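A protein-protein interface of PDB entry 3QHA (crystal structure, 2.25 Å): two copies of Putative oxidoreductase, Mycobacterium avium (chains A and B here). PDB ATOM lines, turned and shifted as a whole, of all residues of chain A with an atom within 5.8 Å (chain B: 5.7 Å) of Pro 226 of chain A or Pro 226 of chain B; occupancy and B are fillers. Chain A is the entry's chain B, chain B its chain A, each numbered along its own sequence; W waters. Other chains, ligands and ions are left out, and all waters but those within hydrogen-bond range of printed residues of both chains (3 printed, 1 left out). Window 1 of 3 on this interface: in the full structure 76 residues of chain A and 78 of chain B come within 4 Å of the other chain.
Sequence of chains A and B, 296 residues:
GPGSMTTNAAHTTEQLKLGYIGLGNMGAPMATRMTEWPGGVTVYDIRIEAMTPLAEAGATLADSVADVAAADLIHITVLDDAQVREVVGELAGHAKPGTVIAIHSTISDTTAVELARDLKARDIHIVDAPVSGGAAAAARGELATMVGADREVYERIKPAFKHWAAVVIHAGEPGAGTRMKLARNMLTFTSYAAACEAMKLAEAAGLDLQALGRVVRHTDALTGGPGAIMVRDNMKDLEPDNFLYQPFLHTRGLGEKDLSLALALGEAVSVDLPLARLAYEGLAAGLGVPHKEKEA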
ATOM      1  N   LEU A 187     -15.072  -9.512   7.354  1.00  0.00           N
ATOM      2  CA  LEU A 187     -14.535 -10.533   8.256  1.00  0.00           C
ATOM      3  C   LEU A 187     -15.623 -11.207   9.080  1.00  0.00           C
ATOM      4  O   LEU A 187     -15.584 -12.427   9.266  1.00  0.00           O
ATOM      5  CB  LEU A 187     -13.483  -9.942   9.200  1.00  0.00           C
ATOM      6  CG  LEU A 187     -12.889 -10.894  10.250  1.00  0.00           C
ATOM      7  CD1 LEU A 187     -12.135 -12.041   9.585  1.00  0.00           C
ATOM      8  CD2 LEU A 187     -11.968 -10.126  11.188  1.00  0.00           C
ATOM      9  N   SER A 191     -16.423 -15.061   8.319  1.00  0.00           N
ATOM     10  CA  SER A 191     -16.169 -15.963   9.446  1.00  0.00           C
ATOM     11  C   SER A 191     -17.423 -16.734   9.874  1.00  0.00           C
ATOM     12  O   SER A 191     -17.318 -17.885  10.297  1.00  0.00           O
ATOM     13  CB  SER A 191     -15.537 -15.224  10.635  1.00  0.00           C
ATOM     14  OG  SER A 191     -16.509 -14.545  11.410  1.00  0.00           O
ATOM     15  N   TYR A 192     -18.602 -16.118   9.760  1.00  0.00           N
ATOM     16  CA  TYR A 192     -19.868 -16.850   9.945  1.00  0.00           C
ATOM     17  C   TYR A 192     -20.028 -17.941   8.881  1.00  0.00           C
ATOM     18  O   TYR A 192     -20.411 -19.066   9.196  1.00  0.00           O
ATOM     19  CB  TYR A 192     -21.090 -15.916   9.901  1.00  0.00           C
ATOM     20  CG  TYR A 192     -21.291 -14.994  11.101  1.00  0.00           C
ATOM     21  CD1 TYR A 192     -20.504 -15.092  12.256  1.00  0.00           C
ATOM     22  CD2 TYR A 192     -22.306 -14.039  11.087  1.00  0.00           C
ATOM     23  CE1 TYR A 192     -20.715 -14.240  13.349  1.00  0.00           C
ATOM     24  CE2 TYR A 192     -22.523 -13.190  12.169  1.00  0.00           C
ATOM     25  CZ  TYR A 192     -21.725 -13.297  13.297  1.00  0.00           C
ATOM     26  OH  TYR A 192     -21.947 -12.457  14.364  1.00  0.00           O
ATOM     27  N   ALA A 195     -17.893 -20.678   9.920  1.00  0.00           N
ATOM     28  CA  ALA A 195     -18.468 -21.367  11.074  1.00  0.00           C
ATOM     29  C   ALA A 195     -19.485 -22.415  10.618  1.00  0.00           C
ATOM     30  O   ALA A 195     -19.473 -23.551  11.094  1.00  0.00           O
ATOM     31  CB  ALA A 195     -19.111 -20.374  12.026  1.00  0.00           C
ATOM     32  N   VAL A 216     -15.970 -23.133  20.812  1.00  0.00           N
ATOM     33  CA  VAL A 216     -15.605 -21.992  19.973  1.00  0.00           C
ATOM     34  C   VAL A 216     -15.700 -20.682  20.753  1.00  0.00           C
ATOM     35  O   VAL A 216     -14.736 -19.917  20.806  1.00  0.00           O
ATOM     36  CB  VAL A 216     -16.498 -21.904  18.711  1.00  0.00           C
ATOM     37  CG1 VAL A 216     -16.269 -20.582  17.971  1.00  0.00           C
ATOM     38  CG2 VAL A 216     -16.230 -23.091  17.789  1.00  0.00           C
ATOM     39  N   ASP A 220     -12.473 -18.452  22.007  1.00  0.00           N
ATOM     40  CA  ASP A 220     -12.358 -17.122  21.403  1.00  0.00           C
ATOM     41  C   ASP A 220     -12.379 -15.994  22.443  1.00  0.00           C
ATOM     42  O   ASP A 220     -11.781 -14.940  22.216  1.00  0.00           O
ATOM     43  CB  ASP A 220     -13.428 -16.901  20.323  1.00  0.00           C
ATOM     44  CG  ASP A 220     -13.039 -17.513  18.980  1.00  0.00           C
ATOM     45  OD1 ASP A 220     -11.843 -17.813  18.786  1.00  0.00           O
ATOM     46  OD2 ASP A 220     -13.925 -17.694  18.117  1.00  0.00           O
ATOM     47  N   GLY A 224      -8.936 -14.109  21.866  1.00  0.00           N
ATOM     48  CA  GLY A 224      -9.277 -12.835  21.235  1.00  0.00           C
ATOM     49  C   GLY A 224     -10.030 -12.981  19.923  1.00  0.00           C
ATOM     50  O   GLY A 224     -10.663 -12.026  19.464  1.00  0.00           O
ATOM     51  N   GLY A 225      -9.962 -14.163  19.310  1.00  0.00           N
ATOM     52  CA  GLY A 225     -10.655 -14.425  18.047  1.00  0.00           C
ATOM     53  C   GLY A 225      -9.790 -14.118  16.833  1.00  0.00           C
ATOM     54  O   GLY A 225      -8.581 -13.926  16.966  1.00  0.00           O
ATOM     55  N   PRO A 226     -10.406 -14.050  15.637  1.00  0.00           N
ATOM     56  CA  PRO A 226      -9.679 -13.751  14.393  1.00  0.00           C
ATOM     57  C   PRO A 226      -8.861 -12.462  14.467  1.00  0.00           C
ATOM     58  O   PRO A 226      -7.819 -12.356  13.819  1.00  0.00           O
ATOM     59  CB  PRO A 226     -10.785 -13.599  13.340  1.00  0.00           C
ATOM     60  CG  PRO A 226     -12.039 -14.071  13.968  1.00  0.00           C
ATOM     61  CD  PRO A 226     -11.866 -14.069  15.446  1.00  0.00           C
ATOM     62  N   GLY A 227      -9.340 -11.499  15.253  1.00  0.00           N
ATOM     63  CA  GLY A 227      -8.641 -10.243  15.473  1.00  0.00           C
ATOM     64  C   GLY A 227      -7.242 -10.404  16.038  1.00  0.00           C
ATOM     65  O   GLY A 227      -6.398  -9.529  15.854  1.00  0.00           O
ATOM     66  N   ALA A 228      -6.994 -11.523  16.717  1.00  0.00           N
ATOM     67  CA  ALA A 228      -5.683 -11.811  17.297  1.00  0.00           C
ATOM     68  C   ALA A 228      -4.558 -11.782  16.265  1.00  0.00           C
ATOM     69  O   ALA A 228      -3.422 -11.466  16.599  1.00  0.00           O
ATOM     70  CB  ALA A 228      -5.707 -13.159  18.010  1.00  0.00           C
ATOM     71  N   ILE A 229      -4.875 -12.101  15.013  1.00  0.00           N
ATOM     72  CA  ILE A 229      -3.867 -12.131  13.953  1.00  0.00           C
ATOM     73  C   ILE A 229      -3.684 -10.762  13.286  1.00  0.00           C
ATOM     74  O   ILE A 229      -2.769 -10.583  12.480  1.00  0.00           O
ATOM     75  CB  ILE A 229      -4.218 -13.207  12.883  1.00  0.00           C
ATOM     76  CG1 ILE A 229      -2.945 -13.827  12.300  1.00  0.00           C
ATOM     77  CG2 ILE A 229      -5.101 -12.627  11.784  1.00  0.00           C
ATOM     78  CD1 ILE A 229      -2.184 -14.700  13.281  1.00  0.00           C
ATOM     79  N   MET A 230      -4.539  -9.801  13.632  1.00  0.00           N
ATOM     80  CA  MET A 230      -4.528  -8.485  12.993  1.00  0.00           C
ATOM     81  C   MET A 230      -3.678  -7.523  13.819  1.00  0.00           C
ATOM     82  O   MET A 230      -4.188  -6.596  14.452  1.00  0.00           O
ATOM     83  CB  MET A 230      -5.959  -7.958  12.822  1.00  0.00           C
ATOM     84  CG  MET A 230      -6.898  -8.944  12.132  1.00  0.00           C
ATOM     85  SD  MET A 230      -8.612  -8.379  12.050  1.00  0.00           S
ATOM     86  CE  MET A 230      -8.535  -7.249  10.666  1.00  0.00           C
ATOM     87  N   LEU B 187     -12.207 -23.669  11.518  1.00  0.00           N
ATOM     88  CA  LEU B 187     -12.796 -22.347  11.704  1.00  0.00           C
ATOM     89  C   LEU B 187     -11.733 -21.315  12.080  1.00  0.00           C
ATOM     90  O   LEU B 187     -11.653 -20.257  11.453  1.00  0.00           O
ATOM     91  CB  LEU B 187     -13.911 -22.381  12.761  1.00  0.00           C
ATOM     92  CG  LEU B 187     -14.510 -21.019  13.146  1.00  0.00           C
ATOM     93  CD1 LEU B 187     -15.003 -20.277  11.914  1.00  0.00           C
ATOM     94  CD2 LEU B 187     -15.630 -21.185  14.166  1.00  0.00           C
ATOM     95  N   SER B 191     -10.685 -18.329   9.482  1.00  0.00           N
ATOM     96  CA  SER B 191     -10.992 -16.957   9.885  1.00  0.00           C
ATOM     97  C   SER B 191      -9.722 -16.100   9.969  1.00  0.00           C
ATOM     98  O   SER B 191      -9.781 -14.886   9.760  1.00  0.00           O
ATOM     99  CB  SER B 191     -11.785 -16.923  11.200  1.00  0.00           C
ATOM    100  OG  SER B 191     -10.960 -17.191  12.320  1.00  0.00           O
ATOM    101  N   TYR B 192      -8.581 -16.724  10.261  1.00  0.00           N
ATOM    102  CA  TYR B 192      -7.295 -16.031  10.176  1.00  0.00           C
ATOM    103  C   TYR B 192      -6.996 -15.636   8.732  1.00  0.00           C
ATOM    104  O   TYR B 192      -6.546 -14.519   8.477  1.00  0.00           O
ATOM    105  CB  TYR B 192      -6.147 -16.880  10.746  1.00  0.00           C
ATOM    106  CG  TYR B 192      -6.062 -16.933  12.268  1.00  0.00           C
ATOM    107  CD1 TYR B 192      -6.852 -16.112  13.081  1.00  0.00           C
ATOM    108  CD2 TYR B 192      -5.161 -17.787  12.894  1.00  0.00           C
ATOM    109  CE1 TYR B 192      -6.758 -16.162  14.465  1.00  0.00           C
ATOM    110  CE2 TYR B 192      -5.061 -17.842  14.278  1.00  0.00           C
ATOM    111  CZ  TYR B 192      -5.862 -17.029  15.057  1.00  0.00           C
ATOM    112  OH  TYR B 192      -5.764 -17.079  16.428  1.00  0.00           O
ATOM    113  N   ALA B 195      -9.270 -12.757   8.034  1.00  0.00           N
ATOM    114  CA  ALA B 195      -8.720 -11.559   8.673  1.00  0.00           C
ATOM    115  C   ALA B 195      -7.641 -10.898   7.817  1.00  0.00           C
ATOM    116  O   ALA B 195      -7.639  -9.681   7.653  1.00  0.00           O
ATOM    117  CB  ALA B 195      -8.160 -11.901  10.060  1.00  0.00           C
ATOM    118  N   VAL B 216     -12.004  -5.019  15.767  1.00  0.00           N
ATOM    119  CA  VAL B 216     -12.371  -6.429  15.648  1.00  0.00           C
ATOM    120  C   VAL B 216     -12.287  -7.155  16.990  1.00  0.00           C
ATOM    121  O   VAL B 216     -13.236  -7.830  17.400  1.00  0.00           O
ATOM    122  CB  VAL B 216     -11.467  -7.157  14.625  1.00  0.00           C
ATOM    123  CG1 VAL B 216     -11.667  -8.667  14.704  1.00  0.00           C
ATOM    124  CG2 VAL B 216     -11.733  -6.642  13.209  1.00  0.00           C
ATOM    125  N   ASP B 220     -15.568  -8.452  19.097  1.00  0.00           N
ATOM    126  CA  ASP B 220     -15.692  -9.907  19.273  1.00  0.00           C
ATOM    127  C   ASP B 220     -15.734 -10.322  20.744  1.00  0.00           C
ATOM    128  O   ASP B 220     -16.298 -11.364  21.069  1.00  0.00           O
ATOM    129  CB  ASP B 220     -14.559 -10.658  18.562  1.00  0.00           C
ATOM    130  CG  ASP B 220     -14.775 -10.777  17.063  1.00  0.00           C
ATOM    131  OD1 ASP B 220     -15.909 -10.566  16.583  1.00  0.00           O
ATOM    132  OD2 ASP B 220     -13.799 -11.100  16.358  1.00  0.00           O
ATOM    133  N   GLY B 224     -18.914 -12.192  21.093  1.00  0.00           N
ATOM    134  CA  GLY B 224     -18.551 -13.605  21.214  1.00  0.00           C
ATOM    135  C   GLY B 224     -17.731 -14.139  20.050  1.00  0.00           C
ATOM    136  O   GLY B 224     -17.056 -15.157  20.192  1.00  0.00           O
ATOM    137  N   GLY B 225     -17.792 -13.465  18.902  1.00  0.00           N
ATOM    138  CA  GLY B 225     -17.014 -13.858  17.725  1.00  0.00           C
ATOM    139  C   GLY B 225     -17.769 -14.790  16.789  1.00  0.00           C
ATOM    140  O   GLY B 225     -18.996 -14.868  16.850  1.00  0.00           O
ATOM    141  N   PRO B 226     -17.039 -15.500  15.907  1.00  0.00           N
ATOM    142  CA  PRO B 226     -17.636 -16.419  14.926  1.00  0.00           C
ATOM    143  C   PRO B 226     -18.616 -17.416  15.540  1.00  0.00           C
ATOM    144  O   PRO B 226     -19.609 -17.766  14.905  1.00  0.00           O
ATOM    145  CB  PRO B 226     -16.428 -17.162  14.349  1.00  0.00           C
ATOM    146  CG  PRO B 226     -15.279 -16.252  14.548  1.00  0.00           C
ATOM    147  CD  PRO B 226     -15.578 -15.394  15.745  1.00  0.00           C
ATOM    148  N   GLY B 227     -18.331 -17.857  16.764  1.00  0.00           N
ATOM    149  CA  GLY B 227     -19.204 -18.765  17.507  1.00  0.00           C
ATOM    150  C   GLY B 227     -20.609 -18.244  17.756  1.00  0.00           C
ATOM    151  O   GLY B 227     -21.511 -19.021  18.072  1.00  0.00           O
ATOM    152  N   ALA B 228     -20.791 -16.931  17.621  1.00  0.00           N
ATOM    153  CA  ALA B 228     -22.107 -16.302  17.728  1.00  0.00           C
ATOM    154  C   ALA B 228     -23.152 -16.895  16.779  1.00  0.00           C
ATOM    155  O   ALA B 228     -24.334 -16.918  17.108  1.00  0.00           O
ATOM    156  CB  ALA B 228     -21.989 -14.797  17.492  1.00  0.00           C
ATOM    157  N   ILE B 229     -22.723 -17.367  15.610  1.00  0.00           N
ATOM    158  CA  ILE B 229     -23.654 -17.917  14.615  1.00  0.00           C
ATOM    159  C   ILE B 229     -23.924 -19.412  14.833  1.00  0.00           C
ATOM    160  O   ILE B 229     -24.785 -19.993  14.173  1.00  0.00           O
ATOM    161  CB  ILE B 229     -23.126 -17.674  13.174  1.00  0.00           C
ATOM    162  CG1 ILE B 229     -24.275 -17.630  12.154  1.00  0.00           C
ATOM    163  CG2 ILE B 229     -22.096 -18.735  12.788  1.00  0.00           C
ATOM    164  CD1 ILE B 229     -25.329 -16.570  12.437  1.00  0.00           C
ATOM    165  N   MET B 230     -23.195 -20.019  15.770  1.00  0.00           N
ATOM    166  CA  MET B 230     -23.277 -21.454  16.041  1.00  0.00           C
ATOM    167  C   MET B 230     -24.314 -21.722  17.126  1.00  0.00           C
ATOM    168  O   MET B 230     -23.979 -22.074  18.257  1.00  0.00           O
ATOM    169  CB  MET B 230     -21.898 -21.995  16.449  1.00  0.00           C
ATOM    170  CG  MET B 230     -20.811 -21.717  15.413  1.00  0.00           C
ATOM    171  SD  MET B 230     -19.163 -22.352  15.816  1.00  0.00           S
ATOM    172  CE  MET B 230     -19.192 -23.950  15.013  1.00  0.00           C
HETATM  173  O   HOH W   1     -16.408 -17.179  18.769  1.00  0.00           O
HETATM  174  O   HOH W   2     -20.028 -12.132  16.137  1.00  0.00           O
HETATM  175  O   HOH W   3     -11.306 -11.091  17.060  1.00  0.00           O
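The backbone carbonyl oxygen (O) of Leu 187 of chain A sits close to the side-chain hydroxyl (OG) of Ser 191 of chain A, 3.2 Å away.
The backbone carbonyl oxygen (O) of Asp 220 of chain B sits at hydrogen-bond distance from the backbone NH (N) of Gly 225 of chain B (3.4 Å).
The backbone carbonyl oxygen (O) of Leu 187 of chain B lies within hydrogen-bond range of the side-chain hydroxyl (OG) of Ser 191 of chain B (3.3 Å).
Among the printed residues, pairs that only touch across the chains: Leu 187 of chain A with Ser 191 of chain B, Leu 187 of chain A with Ala 195 of chain B, Leu 187 of chain A with Val 216 of chain B, Ser 191 of chain A with Leu 187 of chain B, Ser 191 of chain A with Pro 226 of chain B, Tyr 192 of chain A with Gly 225 of chain B, Tyr 192 of chain A with Pro 226 of chain B, Tyr 192 of chain A with Ala 228 of chain B, Tyr 192 of chain A with Ile 229 of chain B, Ala 195 of chain A with Leu 187 of chain B, Ala 195 of chain A with Pro 226 of chain B, Ala 195 of chain A with Ile 229 of chain B, Ala 195 of chain A with Met 230 of chain B, Val 216 of chain A with Leu 187 of chain B, Val 216 of chain A with Gly 227 of chain B, Val 216 of chain A with Met 230 of chain B, Asp 220 of chain A with Pro 226 of chain B, Gly 225 of chain A with Tyr 192 of chain B, Pro 226 of chain A with Ser 191 of chain B, Pro 226 of chain A with Tyr 192 of chain B, Pro 226 of chain A with Ala 195 of chain B, Pro 226 of chain A with Asp 220 of chain B, Pro 226 of chain A with Pro 226 of chain B, Gly 227 of chain A with Val 216 of chain B, Ile 229 of chain A with Tyr 192 of chain B, Ile 229 of chain A with Ala 195 of chain B, Met 230 of chain A with Ala 195 of chain B and Met 230 of chain A with Val 216 of chain B.
Printed residues of chain B within 4 Å of Tyr 192 of chain A: Gly 225 (3.95 Å), Pro 226 (3.9 Å), Ala 228 (3.9 Å) and Ile 229 (3.8 Å).
Of the printed residues of chain B, Met 230 of chain A touches Ala 195 and Val 216.
Of the printed residues of chain A, Val 216 of chain B touches Leu 187 (3.8 Å), Gly 227 (3.5 Å) and Met 230 (3.8 Å).
Of chain A, only Ser 191 (3.8 Å), Tyr 192 (3.9 Å), Ala 195 (3.9 Å), Asp 220 (3.7 Å) and Pro 226 (3.9 Å) come within 4 Å of Pro 226 of chain B.
The nearest printed residue of chain A that does not touch Ser 191 of chain B is Ser 191 of chain A (4.2 Å).
Hydrophobic or aromatic side chains of chain B that line the printed part of chain A: Leu 187, Tyr 192, Ala 195, Val 216, Pro 226, Ala 228, Ile 229 and Met 230.
Among the printed residues, no Asp or Glu carboxylate lies within 4 Å of a Lys or Arg side-chain nitrogen of the other chain.
Ser 191 of chain A touches Pro 226 of chain B, and with the chains exchanged Pro 226 of chain A touches Ser 191 of chain B.
Tyr 192 of chain A touches Gly 225 of chain B, and with the chains exchanged Gly 225 of chain A touches Tyr 192 of chain B.
Tyr 192 of chain A touches Pro 226 of chain B, and with the chains exchanged Pro 226 of chain A touches Tyr 192 of chain B.
Val 216 of chain A touches Met 230 of chain B, and with the chains exchanged Met 230 of chain A touches Val 216 of chain B.
13 positions are printed for both chains.
Of the 28 pairs that touch across the chains among the printed residues, 27 have their exchanged pair printed and touching as well.
Water W1 lies within hydrogen-bond range of O of Gly 224 of chain B (2.6 Å), OD2 of Asp 220 of chain A (2.6 Å) and N of Gly 227 of chain B (2.9 Å).
Water W3 lies within hydrogen-bond range of OD2 of Asp 220 of chain B, O of Gly 224 of chain A and N of Gly 227 of chain A.
Water W2 bridges OH of Tyr 192 of chain A (2.6 Å) and O of Gly 225 of chain B (3.0 Å).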
